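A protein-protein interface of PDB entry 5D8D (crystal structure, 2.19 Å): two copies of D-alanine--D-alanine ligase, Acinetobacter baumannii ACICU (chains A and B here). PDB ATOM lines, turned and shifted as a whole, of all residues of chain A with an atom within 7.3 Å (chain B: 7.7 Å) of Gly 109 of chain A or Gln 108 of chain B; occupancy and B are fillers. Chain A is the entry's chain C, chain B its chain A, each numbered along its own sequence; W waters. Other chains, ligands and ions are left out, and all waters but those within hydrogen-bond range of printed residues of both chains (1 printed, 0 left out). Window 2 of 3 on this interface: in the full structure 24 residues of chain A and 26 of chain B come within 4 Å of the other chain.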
ATOM      1  N   THR A 103      27.994  -0.883 -20.864  1.00  0.00           N
ATOM      2  CA  THR A 103      26.845  -0.450 -21.672  1.00  0.00           C
ATOM      3  C   THR A 103      25.663   0.031 -20.795  1.00  0.00           C
ATOM      4  O   THR A 103      25.055   1.084 -21.052  1.00  0.00           O
ATOM      5  CB  THR A 103      26.344  -1.583 -22.601  1.00  0.00           C
ATOM      6  OG1 THR A 103      27.432  -2.097 -23.384  1.00  0.00           O
ATOM      7  CG2 THR A 103      25.249  -1.061 -23.538  1.00  0.00           C
ATOM      8  N   LYS A 104      25.323  -0.746 -19.774  1.00  0.00           N
ATOM      9  CA  LYS A 104      24.188  -0.353 -18.920  1.00  0.00           C
ATOM     10  C   LYS A 104      24.534   0.904 -18.101  1.00  0.00           C
ATOM     11  O   LYS A 104      23.709   1.847 -18.007  1.00  0.00           O
ATOM     12  CB  LYS A 104      23.718  -1.533 -18.067  1.00  0.00           C
ATOM     13  CG  LYS A 104      22.991  -2.584 -18.894  1.00  0.00           C
ATOM     14  CD  LYS A 104      22.895  -3.919 -18.166  1.00  0.00           C
ATOM     15  CE  LYS A 104      22.029  -3.825 -16.914  1.00  0.00           C
ATOM     16  NZ  LYS A 104      20.686  -3.217 -17.135  1.00  0.00           N
ATOM     17  N   GLN A 105      25.766   0.939 -17.575  1.00  0.00           N
ATOM     18  CA  GLN A 105      26.285   2.147 -16.909  1.00  0.00           C
ATOM     19  C   GLN A 105      26.112   3.365 -17.772  1.00  0.00           C
ATOM     20  O   GLN A 105      25.593   4.364 -17.298  1.00  0.00           O
ATOM     21  CB  GLN A 105      27.758   2.019 -16.452  1.00  0.00           C
ATOM     22  CG  GLN A 105      27.853   1.526 -15.015  1.00  0.00           C
ATOM     23  CD  GLN A 105      29.179   0.906 -14.622  1.00  0.00           C
ATOM     24  OE1 GLN A 105      29.994   0.480 -15.456  1.00  0.00           O
ATOM     25  NE2 GLN A 105      29.405   0.852 -13.319  1.00  0.00           N
ATOM     26  N   ILE A 106      26.493   3.300 -19.043  1.00  0.00           N
ATOM     27  CA  ILE A 106      26.454   4.541 -19.805  1.00  0.00           C
ATOM     28  C   ILE A 106      24.979   4.924 -20.023  1.00  0.00           C
ATOM     29  O   ILE A 106      24.605   6.125 -20.021  1.00  0.00           O
ATOM     30  CB  ILE A 106      27.393   4.609 -21.069  1.00  0.00           C
ATOM     31  CG1 ILE A 106      26.611   4.606 -22.360  1.00  0.00           C
ATOM     32  CG2 ILE A 106      28.569   3.624 -21.085  1.00  0.00           C
ATOM     33  CD1 ILE A 106      26.302   5.998 -22.819  1.00  0.00           C
ATOM     34  N   TRP A 107      24.148   3.887 -20.166  1.00  0.00           N
ATOM     35  CA  TRP A 107      22.712   4.057 -20.331  1.00  0.00           C
ATOM     36  C   TRP A 107      22.082   4.680 -19.081  1.00  0.00           C
ATOM     37  O   TRP A 107      21.334   5.673 -19.220  1.00  0.00           O
ATOM     38  CB  TRP A 107      22.020   2.731 -20.709  1.00  0.00           C
ATOM     39  CG  TRP A 107      22.164   2.288 -22.191  1.00  0.00           C
ATOM     40  CD1 TRP A 107      22.476   3.072 -23.298  1.00  0.00           C
ATOM     41  CD2 TRP A 107      21.954   0.973 -22.691  1.00  0.00           C
ATOM     42  NE1 TRP A 107      22.501   2.301 -24.432  1.00  0.00           N
ATOM     43  CE2 TRP A 107      22.165   1.015 -24.091  1.00  0.00           C
ATOM     44  CE3 TRP A 107      21.596  -0.238 -22.091  1.00  0.00           C
ATOM     45  CZ2 TRP A 107      22.033  -0.111 -24.896  1.00  0.00           C
ATOM     46  CZ3 TRP A 107      21.472  -1.357 -22.885  1.00  0.00           C
ATOM     47  CH2 TRP A 107      21.687  -1.282 -24.284  1.00  0.00           C
ATOM     48  N   GLN A 108      22.405   4.165 -17.881  1.00  0.00           N
ATOM     49  CA  GLN A 108      21.963   4.852 -16.634  1.00  0.00           C
ATOM     50  C   GLN A 108      22.328   6.322 -16.736  1.00  0.00           C
ATOM     51  O   GLN A 108      21.477   7.197 -16.611  1.00  0.00           O
ATOM     52  CB  GLN A 108      22.579   4.253 -15.373  1.00  0.00           C
ATOM     53  CG  GLN A 108      22.041   2.873 -15.040  1.00  0.00           C
ATOM     54  CD  GLN A 108      22.891   2.104 -14.036  1.00  0.00           C
ATOM     55  OE1 GLN A 108      24.100   2.360 -13.861  1.00  0.00           O
ATOM     56  NE2 GLN A 108      22.258   1.132 -13.371  1.00  0.00           N
ATOM     57  N   GLY A 109      23.583   6.570 -17.091  1.00  0.00           N
ATOM     58  CA  GLY A 109      24.127   7.903 -17.137  1.00  0.00           C
ATOM     59  C   GLY A 109      23.530   8.813 -18.165  1.00  0.00           C
ATOM     60  O   GLY A 109      23.702  10.008 -18.042  1.00  0.00           O
ATOM     61  N   SER A 110      22.857   8.279 -19.188  1.00  0.00           N
ATOM     62  CA  SER A 110      22.152   9.123 -20.181  1.00  0.00           C
ATOM     63  C   SER A 110      20.651   9.239 -19.892  1.00  0.00           C
ATOM     64  O   SER A 110      19.913   9.741 -20.749  1.00  0.00           O
ATOM     65  CB  SER A 110      22.354   8.595 -21.615  1.00  0.00           C
ATOM     66  OG  SER A 110      23.633   8.012 -21.800  1.00  0.00           O
ATOM     67  N   ASP A 111      20.219   8.801 -18.695  1.00  0.00           N
ATOM     68  CA  ASP A 111      18.793   8.793 -18.255  1.00  0.00           C
ATOM     69  C   ASP A 111      17.908   7.912 -19.154  1.00  0.00           C
ATOM     70  O   ASP A 111      16.822   8.303 -19.581  1.00  0.00           O
ATOM     71  CB  ASP A 111      18.216  10.226 -18.099  1.00  0.00           C
ATOM     72  CG  ASP A 111      18.873  11.003 -16.962  1.00  0.00           C
ATOM     73  OD1 ASP A 111      18.877  10.478 -15.828  1.00  0.00           O
ATOM     74  OD2 ASP A 111      19.385  12.127 -17.197  1.00  0.00           O
ATOM     75  N   LEU A 112      18.407   6.712 -19.416  1.00  0.00           N
ATOM     76  CA  LEU A 112      17.727   5.740 -20.209  1.00  0.00           C
ATOM     77  C   LEU A 112      17.490   4.544 -19.314  1.00  0.00           C
ATOM     78  O   LEU A 112      18.396   4.137 -18.574  1.00  0.00           O
ATOM     79  CB  LEU A 112      18.563   5.316 -21.417  1.00  0.00           C
ATOM     80  CG  LEU A 112      18.376   6.000 -22.769  1.00  0.00           C
ATOM     81  CD1 LEU A 112      17.808   7.406 -22.680  1.00  0.00           C
ATOM     82  CD2 LEU A 112      19.698   6.007 -23.542  1.00  0.00           C
ATOM     83  N   THR A 114      17.014   0.956 -17.712  1.00  0.00           N
ATOM     84  CA  THR A 114      17.629  -0.356 -17.768  1.00  0.00           C
ATOM     85  C   THR A 114      17.467  -0.984 -16.379  1.00  0.00           C
ATOM     86  O   THR A 114      17.404  -0.274 -15.383  1.00  0.00           O
ATOM     87  CB  THR A 114      19.133  -0.274 -18.247  1.00  0.00           C
ATOM     88  OG1 THR A 114      19.711  -1.584 -18.343  1.00  0.00           O
ATOM     89  CG2 THR A 114      19.996   0.537 -17.310  1.00  0.00           C
ATOM     90  N   VAL B 101      32.651  12.621 -21.230  1.00  0.00           N
ATOM     91  CA  VAL B 101      31.282  12.343 -20.785  1.00  0.00           C
ATOM     92  C   VAL B 101      31.117  10.877 -20.474  1.00  0.00           C
ATOM     93  O   VAL B 101      30.493  10.560 -19.436  1.00  0.00           O
ATOM     94  CB  VAL B 101      30.118  12.907 -21.650  1.00  0.00           C
ATOM     95  CG1 VAL B 101      30.575  13.952 -22.661  1.00  0.00           C
ATOM     96  CG2 VAL B 101      29.237  11.815 -22.256  1.00  0.00           C
ATOM     97  N   LYS B 102      31.686   9.984 -21.308  1.00  0.00           N
ATOM     98  CA  LYS B 102      31.519   8.541 -21.050  1.00  0.00           C
ATOM     99  C   LYS B 102      32.227   8.108 -19.799  1.00  0.00           C
ATOM    100  O   LYS B 102      31.724   7.261 -19.075  1.00  0.00           O
ATOM    101  CB  LYS B 102      31.915   7.669 -22.250  1.00  0.00           C
ATOM    102  CG  LYS B 102      30.944   7.818 -23.411  1.00  0.00           C
ATOM    103  CD  LYS B 102      31.165   6.775 -24.471  1.00  0.00           C
ATOM    104  CE  LYS B 102      30.194   6.957 -25.627  1.00  0.00           C
ATOM    105  NZ  LYS B 102      30.567   8.083 -26.504  1.00  0.00           N
ATOM    106  N   THR B 103      33.387   8.708 -19.528  1.00  0.00           N
ATOM    107  CA  THR B 103      34.082   8.522 -18.251  1.00  0.00           C
ATOM    108  C   THR B 103      33.175   8.913 -17.053  1.00  0.00           C
ATOM    109  O   THR B 103      33.086   8.190 -16.069  1.00  0.00           O
ATOM    110  CB  THR B 103      35.393   9.324 -18.234  1.00  0.00           C
ATOM    111  OG1 THR B 103      36.294   8.806 -19.219  1.00  0.00           O
ATOM    112  CG2 THR B 103      36.081   9.203 -16.894  1.00  0.00           C
ATOM    113  N   LYS B 104      32.528  10.065 -17.140  1.00  0.00           N
ATOM    114  CA  LYS B 104      31.675  10.541 -16.035  1.00  0.00           C
ATOM    115  C   LYS B 104      30.411   9.692 -15.854  1.00  0.00           C
ATOM    116  O   LYS B 104      29.995   9.443 -14.729  1.00  0.00           O
ATOM    117  CB  LYS B 104      31.279  11.996 -16.225  1.00  0.00           C
ATOM    118  CG  LYS B 104      32.394  12.984 -15.991  1.00  0.00           C
ATOM    119  CD  LYS B 104      32.072  14.278 -16.738  1.00  0.00           C
ATOM    120  CE  LYS B 104      32.395  15.546 -15.984  1.00  0.00           C
ATOM    121  NZ  LYS B 104      31.444  15.819 -14.861  1.00  0.00           N
ATOM    122  N   GLN B 105      29.830   9.223 -16.957  1.00  0.00           N
ATOM    123  CA  GLN B 105      28.681   8.357 -16.869  1.00  0.00           C
ATOM    124  C   GLN B 105      29.095   7.086 -16.190  1.00  0.00           C
ATOM    125  O   GLN B 105      28.415   6.637 -15.274  1.00  0.00           O
ATOM    126  CB  GLN B 105      28.104   8.075 -18.227  1.00  0.00           C
ATOM    127  CG  GLN B 105      27.569   9.318 -18.910  1.00  0.00           C
ATOM    128  CD  GLN B 105      27.216   9.166 -20.385  1.00  0.00           C
ATOM    129  OE1 GLN B 105      26.350   9.887 -20.873  1.00  0.00           O
ATOM    130  NE2 GLN B 105      27.877   8.263 -21.105  1.00  0.00           N
ATOM    131  N   ILE B 106      30.224   6.508 -16.586  1.00  0.00           N
ATOM    132  CA  ILE B 106      30.755   5.367 -15.824  1.00  0.00           C
ATOM    133  C   ILE B 106      30.931   5.689 -14.332  1.00  0.00           C
ATOM    134  O   ILE B 106      30.622   4.850 -13.447  1.00  0.00           O
ATOM    135  CB  ILE B 106      32.088   4.845 -16.373  1.00  0.00           C
ATOM    136  CG1 ILE B 106      31.963   4.365 -17.829  1.00  0.00           C
ATOM    137  CG2 ILE B 106      32.600   3.692 -15.517  1.00  0.00           C
ATOM    138  CD1 ILE B 106      30.865   3.370 -18.097  1.00  0.00           C
ATOM    139  N   TRP B 107      31.428   6.894 -14.047  1.00  0.00           N
ATOM    140  CA  TRP B 107      31.554   7.356 -12.665  1.00  0.00           C
ATOM    141  C   TRP B 107      30.189   7.624 -11.941  1.00  0.00           C
ATOM    142  O   TRP B 107      30.024   7.174 -10.803  1.00  0.00           O
ATOM    143  CB  TRP B 107      32.502   8.565 -12.579  1.00  0.00           C
ATOM    144  CG  TRP B 107      33.944   8.253 -12.838  1.00  0.00           C
ATOM    145  CD1 TRP B 107      34.580   7.033 -12.734  1.00  0.00           C
ATOM    146  CD2 TRP B 107      34.936   9.180 -13.222  1.00  0.00           C
ATOM    147  NE1 TRP B 107      35.898   7.161 -13.056  1.00  0.00           N
ATOM    148  CE2 TRP B 107      36.142   8.470 -13.367  1.00  0.00           C
ATOM    149  CE3 TRP B 107      34.924  10.555 -13.475  1.00  0.00           C
ATOM    150  CZ2 TRP B 107      37.326   9.088 -13.734  1.00  0.00           C
ATOM    151  CZ3 TRP B 107      36.110  11.169 -13.841  1.00  0.00           C
ATOM    152  CH2 TRP B 107      37.288  10.436 -13.962  1.00  0.00           C
ATOM    153  N   GLN B 108      29.233   8.315 -12.577  1.00  0.00           N
ATOM    154  CA  GLN B 108      27.843   8.426 -12.056  1.00  0.00           C
ATOM    155  C   GLN B 108      27.278   7.053 -11.784  1.00  0.00           C
ATOM    156  O   GLN B 108      26.697   6.799 -10.746  1.00  0.00           O
ATOM    157  CB  GLN B 108      26.943   9.122 -13.057  1.00  0.00           C
ATOM    158  CG  GLN B 108      27.025  10.632 -12.982  1.00  0.00           C
ATOM    159  CD  GLN B 108      26.513  11.355 -14.226  1.00  0.00           C
ATOM    160  OE1 GLN B 108      26.184  10.741 -15.262  1.00  0.00           O
ATOM    161  NE2 GLN B 108      26.456  12.692 -14.134  1.00  0.00           N
ATOM    162  N   GLY B 109      27.547   6.144 -12.708  1.00  0.00           N
ATOM    163  CA  GLY B 109      27.052   4.817 -12.631  1.00  0.00           C
ATOM    164  C   GLY B 109      27.694   3.940 -11.605  1.00  0.00           C
ATOM    165  O   GLY B 109      27.262   2.805 -11.462  1.00  0.00           O
ATOM    166  N   SER B 110      28.736   4.412 -10.927  1.00  0.00           N
ATOM    167  CA  SER B 110      29.424   3.601  -9.919  1.00  0.00           C
ATOM    168  C   SER B 110      29.388   4.271  -8.558  1.00  0.00           C
ATOM    169  O   SER B 110      30.157   3.892  -7.668  1.00  0.00           O
ATOM    170  CB  SER B 110      30.876   3.355 -10.327  1.00  0.00           C
ATOM    171  OG  SER B 110      30.986   3.147 -11.726  1.00  0.00           O
ATOM    172  N   ASP B 111      28.493   5.254  -8.405  1.00  0.00           N
ATOM    173  CA  ASP B 111      28.268   5.965  -7.142  1.00  0.00           C
ATOM    174  C   ASP B 111      29.474   6.812  -6.693  1.00  0.00           C
ATOM    175  O   ASP B 111      29.755   6.948  -5.500  1.00  0.00           O
ATOM    176  CB  ASP B 111      27.783   4.980  -6.053  1.00  0.00           C
ATOM    177  CG  ASP B 111      26.461   5.419  -5.430  1.00  0.00           C
ATOM    178  OD1 ASP B 111      26.412   6.560  -4.899  1.00  0.00           O
ATOM    179  OD2 ASP B 111      25.475   4.636  -5.502  1.00  0.00           O
ATOM    180  N   LEU B 112      30.150   7.407  -7.673  1.00  0.00           N
ATOM    181  CA  LEU B 112      31.386   8.160  -7.487  1.00  0.00           C
ATOM    182  C   LEU B 112      31.032   9.596  -7.873  1.00  0.00           C
ATOM    183  O   LEU B 112      30.338   9.820  -8.878  1.00  0.00           O
ATOM    184  CB  LEU B 112      32.509   7.592  -8.384  1.00  0.00           C
ATOM    185  CG  LEU B 112      33.548   6.604  -7.829  1.00  0.00           C
ATOM    186  CD1 LEU B 112      33.071   5.761  -6.657  1.00  0.00           C
ATOM    187  CD2 LEU B 112      34.066   5.688  -8.907  1.00  0.00           C
ATOM    188  N   PRO B 113      31.502  10.576  -7.095  1.00  0.00           N
ATOM    189  CA  PRO B 113      31.094  11.958  -7.355  1.00  0.00           C
ATOM    190  C   PRO B 113      31.796  12.619  -8.540  1.00  0.00           C
ATOM    191  O   PRO B 113      33.001  12.488  -8.701  1.00  0.00           O
ATOM    192  CB  PRO B 113      31.484  12.666  -6.067  1.00  0.00           C
ATOM    193  CG  PRO B 113      32.715  11.930  -5.621  1.00  0.00           C
ATOM    194  CD  PRO B 113      32.524  10.494  -6.037  1.00  0.00           C
ATOM    195  N   THR B 114      31.029  13.359  -9.320  1.00  0.00           N
ATOM    196  CA  THR B 114      31.531  14.065 -10.465  1.00  0.00           C
ATOM    197  C   THR B 114      30.534  15.179 -10.758  1.00  0.00           C
ATOM    198  O   THR B 114      29.374  15.076 -10.377  1.00  0.00           O
ATOM    199  CB  THR B 114      31.704  13.106 -11.661  1.00  0.00           C
ATOM    200  OG1 THR B 114      32.319  13.796 -12.740  1.00  0.00           O
ATOM    201  CG2 THR B 114      30.385  12.545 -12.144  1.00  0.00           C
ATOM    202  N   ALA B 115      30.973  16.266 -11.387  1.00  0.00           N
ATOM    203  CA  ALA B 115      30.099  17.425 -11.531  1.00  0.00           C
ATOM    204  C   ALA B 115      28.991  17.187 -12.564  1.00  0.00           C
ATOM    205  O   ALA B 115      29.243  16.593 -13.622  1.00  0.00           O
ATOM    206  CB  ALA B 115      30.898  18.673 -11.888  1.00  0.00           C
ATOM    207  N   PRO B 116      27.760  17.657 -12.268  1.00  0.00           N
ATOM    208  CA  PRO B 116      26.736  17.654 -13.320  1.00  0.00           C
ATOM    209  C   PRO B 116      27.253  18.303 -14.608  1.00  0.00           C
ATOM    210  O   PRO B 116      28.158  19.186 -14.565  1.00  0.00           O
ATOM    211  CB  PRO B 116      25.600  18.490 -12.715  1.00  0.00           C
ATOM    212  CG  PRO B 116      25.774  18.355 -11.235  1.00  0.00           C
ATOM    213  CD  PRO B 116      27.247  18.203 -10.990  1.00  0.00           C
ATOM    214  N   TYR B 117      26.690  17.863 -15.735  1.00  0.00           N
ATOM    215  CA  TYR B 117      27.069  18.394 -17.036  1.00  0.00           C
ATOM    216  C   TYR B 117      25.892  18.303 -18.000  1.00  0.00           C
ATOM    217  O   TYR B 117      24.883  17.690 -17.678  1.00  0.00           O
ATOM    218  CB  TYR B 117      28.255  17.585 -17.590  1.00  0.00           C
ATOM    219  CG  TYR B 117      27.872  16.147 -17.813  1.00  0.00           C
ATOM    220  CD1 TYR B 117      27.891  15.233 -16.751  1.00  0.00           C
ATOM    221  CD2 TYR B 117      27.425  15.709 -19.078  1.00  0.00           C
ATOM    222  CE1 TYR B 117      27.488  13.920 -16.934  1.00  0.00           C
ATOM    223  CE2 TYR B 117      27.013  14.393 -19.274  1.00  0.00           C
ATOM    224  CZ  TYR B 117      27.050  13.498 -18.206  1.00  0.00           C
ATOM    225  OH  TYR B 117      26.660  12.190 -18.387  1.00  0.00           O
ATOM    226  N   ARG B 118      26.046  18.876 -19.191  1.00  0.00           N
ATOM    227  CA  ARG B 118      25.077  18.741 -20.272  1.00  0.00           C
ATOM    228  C   ARG B 118      25.768  18.774 -21.642  1.00  0.00           C
ATOM    229  O   ARG B 118      26.564  19.678 -21.934  1.00  0.00           O
ATOM    230  CB  ARG B 118      24.011  19.860 -20.197  1.00  0.00           C
ATOM    231  CG  ARG B 118      22.997  19.762 -19.052  1.00  0.00           C
ATOM    232  CD  ARG B 118      22.087  18.522 -19.099  1.00  0.00           C
ATOM    233  NE  ARG B 118      21.939  17.896 -17.776  1.00  0.00           N
ATOM    234  CZ  ARG B 118      21.057  18.233 -16.823  1.00  0.00           C
ATOM    235  NH1 ARG B 118      20.167  19.208 -16.991  1.00  0.00           N
ATOM    236  NH2 ARG B 118      21.059  17.567 -15.666  1.00  0.00           N
ATOM    237  N   ILE B 119      25.432  17.810 -22.495  1.00  0.00           N
ATOM    238  CA  ILE B 119      26.007  17.735 -23.842  1.00  0.00           C
ATOM    239  C   ILE B 119      25.295  18.826 -24.639  1.00  0.00           C
ATOM    240  O   ILE B 119      24.063  18.997 -24.507  1.00  0.00           O
ATOM    241  CB  ILE B 119      25.838  16.324 -24.493  1.00  0.00           C
ATOM    242  CG1 ILE B 119      26.413  15.209 -23.590  1.00  0.00           C
ATOM    243  CG2 ILE B 119      26.535  16.270 -25.846  1.00  0.00           C
ATOM    244  CD1 ILE B 119      25.845  13.816 -23.822  1.00  0.00           C
ATOM    245  N   LEU B 266      35.593  14.262  -9.105  1.00  0.00           N
ATOM    246  CA  LEU B 266      36.393  13.671 -10.165  1.00  0.00           C
ATOM    247  C   LEU B 266      36.215  14.373 -11.509  1.00  0.00           C
ATOM    248  O   LEU B 266      35.090  14.630 -11.935  1.00  0.00           O
ATOM    249  CB  LEU B 266      36.039  12.221 -10.334  1.00  0.00           C
ATOM    250  CG  LEU B 266      36.333  11.319  -9.149  1.00  0.00           C
ATOM    251  CD1 LEU B 266      35.506  10.062  -9.331  1.00  0.00           C
ATOM    252  CD2 LEU B 266      37.788  10.944  -9.057  1.00  0.00           C
HETATM  253  O   HOH W   1      32.011   0.336 -11.931  1.00  0.00           O
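OG of Ser 110 of chain B lies within hydrogen-bond range of NE2 of Gln 105 of chain A, at 3.2 Å. OE1 of Gln 105 of chain B is in hydrogen-bond range of OG of Ser 110 of chain A (3.4 Å). The backbone carbonyl oxygen (O) of Gly 109 of chain B is in hydrogen-bond range of the side-chain amide nitrogen (NE2) of Gln 105 of chain A, 3.4 Å away.
Of the printed residues of chain B, Ile 106 of chain A touches Gln 105 (3.2 Å) and Ile 106 (3.8 Å). Printed residues of chain B within 4 Å of Gln 108 of chain A: Gly 109. Gly 109 of chain A touches just these residues of chain B: Gln 105, Gln 108 and Tyr 117. Printed residues of chain B within 4 Å of Ser 110 of chain A: Gln 105 (3.4 Å). Asp 111 of chain A touches none of the printed residues of chain B. Gln 108 of chain B touches just one residue of chain A: Gly 109 (3.8 Å). Of the printed residues of chain A, Gly 109 of chain B touches Gln 105 and Gln 108. Ala 115 of chain B touches none of the printed residues of chain A. The nearest residue of chain B that does not touch Gly 109 of chain A is Gly 109 of chain B (5.9 Å). The nearest residue of chain A that does not touch Gln 108 of chain B is Ser 110 of chain A (5.7 Å).
O of Ile 106 of chain A lies within hydrogen-bond range of OG of Ser 110 of chain A. The side-chain hydroxyl (OG) of Ser 110 of chain B lies within hydrogen-bond range of the backbone carbonyl oxygen (O) of Ile 106 of chain B (2.4 Å). The side-chain hydroxyl of Tyr 117 of chain B lies close to the side-chain amide oxygen of Gln 105 of chain B, at 3.4 Å. OE1 of Gln 108 of chain B is in hydrogen-bond range of OH of Tyr 117 of chain B (3.5 Å).
Gln 105 of chain A touches Ile 106 of chain B. CD1 of Ile 106 of chain A touches NE2 of Gln 105 of chain B (3.2 Å). CD1 of Ile 106 of chain B touches CG2 of Ile 106 of chain A, at 3.8 Å. O of Gly 109 of chain B touches OE1 of Gln 108 of chain A (3.99 Å). Gln 105 of chain B touches Gly 109 of chain A (OE1 to O, 3.9 Å). Gln 108 of chain B touches Gly 109 of chain A. Tyr 117 of chain B touches Gly 109 of chain A.
Of the 20 printed residues of chain B, 6 touch a printed residue of chain A. Hydrophobic or aromatic side chains of chain B that line the printed part of chain A: Ile 106 and Tyr 117. Among the printed residues, 10 pairs touch across the chains.
Gln 105 of chain A touches Ile 106 of chain B, and with the chains exchanged Ile 106 of chain A touches Gln 105 of chain B. Gln 105 of chain A touches Gly 109 of chain B, and with the chains exchanged Gly 109 of chain A touches Gln 105 of chain B. Ile 106 of chain B touches its own counterpart, Ile 106 of chain A. Gln 108 of chain A touches Gly 109 of chain B, and with the chains exchanged Gly 109 of chain A touches Gln 108 of chain B. Positions printed for both chains: 103, 104, 105, 106, 107, 108, 109, 110, 111, 112 and 114.
Water W1 bridges NE2 of Gln 105 of chain A and OG of Ser 110 of chain B.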
